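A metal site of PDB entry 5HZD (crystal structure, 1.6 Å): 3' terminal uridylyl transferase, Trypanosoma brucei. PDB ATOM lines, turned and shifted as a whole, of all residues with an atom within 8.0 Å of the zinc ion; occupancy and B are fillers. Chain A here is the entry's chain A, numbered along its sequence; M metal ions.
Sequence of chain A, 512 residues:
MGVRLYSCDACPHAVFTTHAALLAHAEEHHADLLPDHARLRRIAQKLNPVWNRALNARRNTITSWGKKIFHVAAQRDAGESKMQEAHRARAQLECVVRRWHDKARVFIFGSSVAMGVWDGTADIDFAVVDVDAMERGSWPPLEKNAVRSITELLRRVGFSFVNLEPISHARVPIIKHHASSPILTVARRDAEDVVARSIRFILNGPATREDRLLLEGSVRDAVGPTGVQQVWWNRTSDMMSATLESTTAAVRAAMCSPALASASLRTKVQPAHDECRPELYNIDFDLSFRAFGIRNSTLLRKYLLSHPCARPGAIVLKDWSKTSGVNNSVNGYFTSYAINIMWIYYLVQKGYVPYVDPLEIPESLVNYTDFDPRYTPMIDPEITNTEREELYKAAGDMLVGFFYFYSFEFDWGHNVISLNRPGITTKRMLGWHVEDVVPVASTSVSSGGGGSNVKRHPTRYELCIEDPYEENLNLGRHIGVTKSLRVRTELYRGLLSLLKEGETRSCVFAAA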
ATOM      1  N   SER A   7       5.490  14.522 -25.027  1.00  0.00           N
ATOM      2  CA  SER A   7       6.424  13.973 -24.065  1.00  0.00           C
ATOM      3  C   SER A   7       7.223  12.845 -24.713  1.00  0.00           C
ATOM      4  O   SER A   7       6.734  12.099 -25.570  1.00  0.00           O
ATOM      5  CB  SER A   7       5.714  13.466 -22.801  1.00  0.00           C
ATOM      6  OG  SER A   7       4.908  12.323 -23.068  1.00  0.00           O
ATOM      7  N   CYS A   8       8.481  12.750 -24.269  1.00  0.00           N
ATOM      8  CA  CYS A   8       9.395  11.690 -24.701  1.00  0.00           C
ATOM      9  C   CYS A   8       9.000  10.345 -24.096  1.00  0.00           C
ATOM     10  O   CYS A   8       8.509  10.280 -22.969  1.00  0.00           O
ATOM     11  CB  CYS A   8      10.810  12.063 -24.283  1.00  0.00           C
ATOM     12  SG  CYS A   8      12.003  10.893 -24.991  1.00  0.00           S
ATOM     13  N   ASP A   9       9.183   9.253 -24.869  1.00  0.00           N
ATOM     14  CA  ASP A   9       8.897   7.898 -24.389  1.00  0.00           C
ATOM     15  C   ASP A   9      10.167   7.174 -23.908  1.00  0.00           C
ATOM     16  O   ASP A   9      10.094   5.990 -23.547  1.00  0.00           O
ATOM     17  CB  ASP A   9       8.218   7.053 -25.475  1.00  0.00           C
ATOM     18  CG  ASP A   9       9.119   6.798 -26.675  1.00  0.00           C
ATOM     19  OD1 ASP A   9      10.076   7.600 -26.883  1.00  0.00           O
ATOM     20  OD2 ASP A   9       8.864   5.806 -27.397  1.00  0.00           O
ATOM     21  N   ALA A  10      11.297   7.861 -23.889  1.00  0.00           N
ATOM     22  CA  ALA A  10      12.590   7.226 -23.586  1.00  0.00           C
ATOM     23  C   ALA A  10      13.270   7.841 -22.379  1.00  0.00           C
ATOM     24  O   ALA A  10      14.294   7.345 -21.907  1.00  0.00           O
ATOM     25  CB  ALA A  10      13.527   7.308 -24.796  1.00  0.00           C
ATOM     26  N   CYS A  11      12.741   8.951 -21.880  1.00  0.00           N
ATOM     27  CA  CYS A  11      13.178   9.463 -20.595  1.00  0.00           C
ATOM     28  C   CYS A  11      11.960  10.054 -19.918  1.00  0.00           C
ATOM     29  O   CYS A  11      10.989  10.410 -20.581  1.00  0.00           O
ATOM     30  CB  CYS A  11      14.322  10.442 -20.749  1.00  0.00           C
ATOM     31  SG  CYS A  11      13.915  11.953 -21.574  1.00  0.00           S
ATOM     32  N   PRO A  12      11.983  10.134 -18.582  1.00  0.00           N
ATOM     33  CA  PRO A  12      10.727  10.450 -17.906  1.00  0.00           C
ATOM     34  C   PRO A  12      10.474  11.939 -17.738  1.00  0.00           C
ATOM     35  O   PRO A  12       9.411  12.293 -17.229  1.00  0.00           O
ATOM     36  CB  PRO A  12      10.916   9.798 -16.531  1.00  0.00           C
ATOM     37  CG  PRO A  12      12.381   9.903 -16.282  1.00  0.00           C
ATOM     38  CD  PRO A  12      13.044   9.727 -17.639  1.00  0.00           C
ATOM     39  N   HIS A  13      11.387  12.795 -18.177  1.00  0.00           N
ATOM     40  CA  HIS A  13      11.319  14.210 -17.830  1.00  0.00           C
ATOM     41  C   HIS A  13      11.124  15.198 -18.989  1.00  0.00           C
ATOM     42  O   HIS A  13      10.866  16.370 -18.755  1.00  0.00           O
ATOM     43  CB  HIS A  13      12.597  14.614 -17.087  1.00  0.00           C
ATOM     44  CG  HIS A  13      13.846  14.425 -17.896  1.00  0.00           C
ATOM     45  ND1 HIS A  13      14.499  13.212 -17.976  1.00  0.00           N
ATOM     46  CD2 HIS A  13      14.541  15.286 -18.662  1.00  0.00           C
ATOM     47  CE1 HIS A  13      15.557  13.344 -18.762  1.00  0.00           C
ATOM     48  NE2 HIS A  13      15.608  14.595 -19.194  1.00  0.00           N
ATOM     49  N   ALA A  14      11.255  14.728 -20.223  1.00  0.00           N
ATOM     50  CA  ALA A  14      11.331  15.665 -21.333  1.00  0.00           C
ATOM     51  C   ALA A  14       9.950  15.923 -21.953  1.00  0.00           C
ATOM     52  O   ALA A  14       9.340  15.035 -22.526  1.00  0.00           O
ATOM     53  CB  ALA A  14      12.332  15.179 -22.386  1.00  0.00           C
ATOM     54  N   VAL A  15       9.473  17.156 -21.762  1.00  0.00           N
ATOM     55  CA  VAL A  15       8.204  17.562 -22.340  1.00  0.00           C
ATOM     56  C   VAL A  15       8.391  18.823 -23.176  1.00  0.00           C
ATOM     57  O   VAL A  15       9.183  19.699 -22.851  1.00  0.00           O
ATOM     58  CB  VAL A  15       7.136  17.796 -21.272  1.00  0.00           C
ATOM     59  CG1 VAL A  15       6.659  16.455 -20.716  1.00  0.00           C
ATOM     60  CG2 VAL A  15       7.671  18.685 -20.178  1.00  0.00           C
ATOM     61  N   PHE A  16       7.664  18.889 -24.276  1.00  0.00           N
ATOM     62  CA  PHE A  16       7.834  20.001 -25.196  1.00  0.00           C
ATOM     63  C   PHE A  16       6.506  20.548 -25.625  1.00  0.00           C
ATOM     64  O   PHE A  16       5.469  19.894 -25.460  1.00  0.00           O
ATOM     65  CB  PHE A  16       8.610  19.501 -26.410  1.00  0.00           C
ATOM     66  CG  PHE A  16       9.910  18.836 -26.042  1.00  0.00           C
ATOM     67  CD1 PHE A  16       9.956  17.476 -25.777  1.00  0.00           C
ATOM     68  CD2 PHE A  16      11.068  19.596 -25.904  1.00  0.00           C
ATOM     69  CE1 PHE A  16      11.158  16.852 -25.392  1.00  0.00           C
ATOM     70  CE2 PHE A  16      12.272  18.991 -25.533  1.00  0.00           C
ATOM     71  CZ  PHE A  16      12.312  17.617 -25.276  1.00  0.00           C
ATOM     72  N   LEU A  22      10.085  17.800 -30.003  1.00  0.00           N
ATOM     73  CA  LEU A  22      10.055  16.406 -29.567  1.00  0.00           C
ATOM     74  C   LEU A  22      10.934  15.540 -30.467  1.00  0.00           C
ATOM     75  O   LEU A  22      11.737  14.747 -29.976  1.00  0.00           O
ATOM     76  CB  LEU A  22       8.630  15.859 -29.558  1.00  0.00           C
ATOM     77  CG  LEU A  22       8.507  14.398 -29.117  1.00  0.00           C
ATOM     78  CD1 LEU A  22       8.763  14.300 -27.617  1.00  0.00           C
ATOM     79  CD2 LEU A  22       7.142  13.813 -29.489  1.00  0.00           C
ATOM     80  N   HIS A  25      14.547  16.267 -30.006  1.00  0.00           N
ATOM     81  CA  HIS A  25      15.017  15.694 -28.747  1.00  0.00           C
ATOM     82  C   HIS A  25      15.313  14.197 -28.935  1.00  0.00           C
ATOM     83  O   HIS A  25      16.314  13.689 -28.420  1.00  0.00           O
ATOM     84  CB  HIS A  25      13.975  15.868 -27.648  1.00  0.00           C
ATOM     85  CG  HIS A  25      14.214  14.999 -26.461  1.00  0.00           C
ATOM     86  ND1 HIS A  25      15.087  15.353 -25.460  1.00  0.00           N
ATOM     87  CD2 HIS A  25      13.711  13.787 -26.119  1.00  0.00           C
ATOM     88  CE1 HIS A  25      15.105  14.401 -24.534  1.00  0.00           C
ATOM     89  NE2 HIS A  25      14.293  13.441 -24.935  1.00  0.00           N
ATOM     90  N   ALA A  26      14.439  13.519 -29.657  1.00  0.00           N
ATOM     91  CA  ALA A  26      14.618  12.067 -29.889  1.00  0.00           C
ATOM     92  C   ALA A  26      15.946  11.752 -30.598  1.00  0.00           C
ATOM     93  O   ALA A  26      16.699  10.876 -30.162  1.00  0.00           O
ATOM     94  CB  ALA A  26      13.439  11.488 -30.616  1.00  0.00           C
ATOM     95  N   HIS A  29      19.099  13.165 -28.104  1.00  0.00           N
ATOM     96  CA  HIS A  29      19.327  12.502 -26.820  1.00  0.00           C
ATOM     97  C   HIS A  29      19.183  10.986 -26.877  1.00  0.00           C
ATOM     98  O   HIS A  29      19.666  10.273 -25.990  1.00  0.00           O
ATOM     99  CB  HIS A  29      18.418  13.092 -25.739  1.00  0.00           C
ATOM    100  CG  HIS A  29      18.829  14.460 -25.281  1.00  0.00           C
ATOM    101  ND1 HIS A  29      18.710  15.578 -26.070  1.00  0.00           N
ATOM    102  CD2 HIS A  29      19.374  14.876 -24.115  1.00  0.00           C
ATOM    103  CE1 HIS A  29      19.159  16.634 -25.417  1.00  0.00           C
ATOM    104  NE2 HIS A  29      19.569  16.233 -24.227  1.00  0.00           N
ATOM    105  N   HIS A  30      18.523  10.481 -27.921  1.00  0.00           N
ATOM    106  CA  HIS A  30      18.241   9.056 -27.957  1.00  0.00           C
ATOM    107  C   HIS A  30      18.674   8.393 -29.230  1.00  0.00           C
ATOM    108  O   HIS A  30      18.088   7.396 -29.654  1.00  0.00           O
ATOM    109  CB  HIS A  30      16.760   8.785 -27.709  1.00  0.00           C
ATOM    110  CG  HIS A  30      16.326   9.211 -26.354  1.00  0.00           C
ATOM    111  ND1 HIS A  30      16.939   8.740 -25.210  1.00  0.00           N
ATOM    112  CD2 HIS A  30      15.416  10.138 -25.950  1.00  0.00           C
ATOM    113  CE1 HIS A  30      16.388   9.311 -24.159  1.00  0.00           C
ATOM    114  NE2 HIS A  30      15.480  10.174 -24.578  1.00  0.00           N
ATOM    115  N   LEU A  33      18.837   4.710 -29.492  1.00  0.00           N
ATOM    116  CA  LEU A  33      17.623   3.930 -29.623  1.00  0.00           C
ATOM    117  C   LEU A  33      17.161   3.847 -31.074  1.00  0.00           C
ATOM    118  O   LEU A  33      16.376   2.969 -31.429  1.00  0.00           O
ATOM    119  CB  LEU A  33      16.527   4.536 -28.740  1.00  0.00           C
ATOM    120  CG  LEU A  33      16.857   4.464 -27.258  1.00  0.00           C
ATOM    121  CD1 LEU A  33      15.718   5.052 -26.452  1.00  0.00           C
ATOM    122  CD2 LEU A  33      17.094   3.004 -26.862  1.00  0.00           C
ATOM    123  N   VAL A 481       7.598   8.389 -29.288  1.00  0.00           N
ATOM    124  CA  VAL A 481       8.416   9.016 -30.323  1.00  0.00           C
ATOM    125  C   VAL A 481       9.649   8.203 -30.729  1.00  0.00           C
ATOM    126  O   VAL A 481       9.888   8.028 -31.937  1.00  0.00           O
ATOM    127  CB  VAL A 481       8.780  10.476 -29.991  1.00  0.00           C
ATOM    128  CG1 VAL A 481       9.681  10.583 -28.766  1.00  0.00           C
ATOM    129  CG2 VAL A 481       9.419  11.154 -31.231  1.00  0.00           C
ATOM    130  N   THR A 482      10.440   7.715 -29.782  1.00  0.00           N
ATOM    131  CA  THR A 482      11.618   6.937 -30.171  1.00  0.00           C
ATOM    132  C   THR A 482      11.202   5.643 -30.834  1.00  0.00           C
ATOM    133  O   THR A 482      11.799   5.245 -31.855  1.00  0.00           O
ATOM    134  CB  THR A 482      12.627   6.710 -28.993  1.00  0.00           C
ATOM    135  OG1 THR A 482      11.994   5.959 -27.954  1.00  0.00           O
ATOM    136  CG2 THR A 482      13.087   8.019 -28.477  1.00  0.00           C
HETATM  137 ZN    ZN M   1      13.908  11.634 -23.915  1.00  0.00          ZN
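The zinc ion is bound by NE2 of His 25 (2.1 Å), NE2 of His 30 (2.2 Å), SG of Cys 8 (2.3 Å) and SG of Cys 11 (2.4 Å).
The side-chain sulfur (SG) of Cys 8 sits close to the backbone NH (N) of Ala 10 (3.3 Å).
The backbone carbonyl oxygen (O) of Ala 14 is in hydrogen-bond range of the backbone NH (N) of Cys 8, at 3.0 Å.
Four residues have an atom within 4 Å of the zinc ion: Cys 8, Cys 11, His 25 and His 30.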
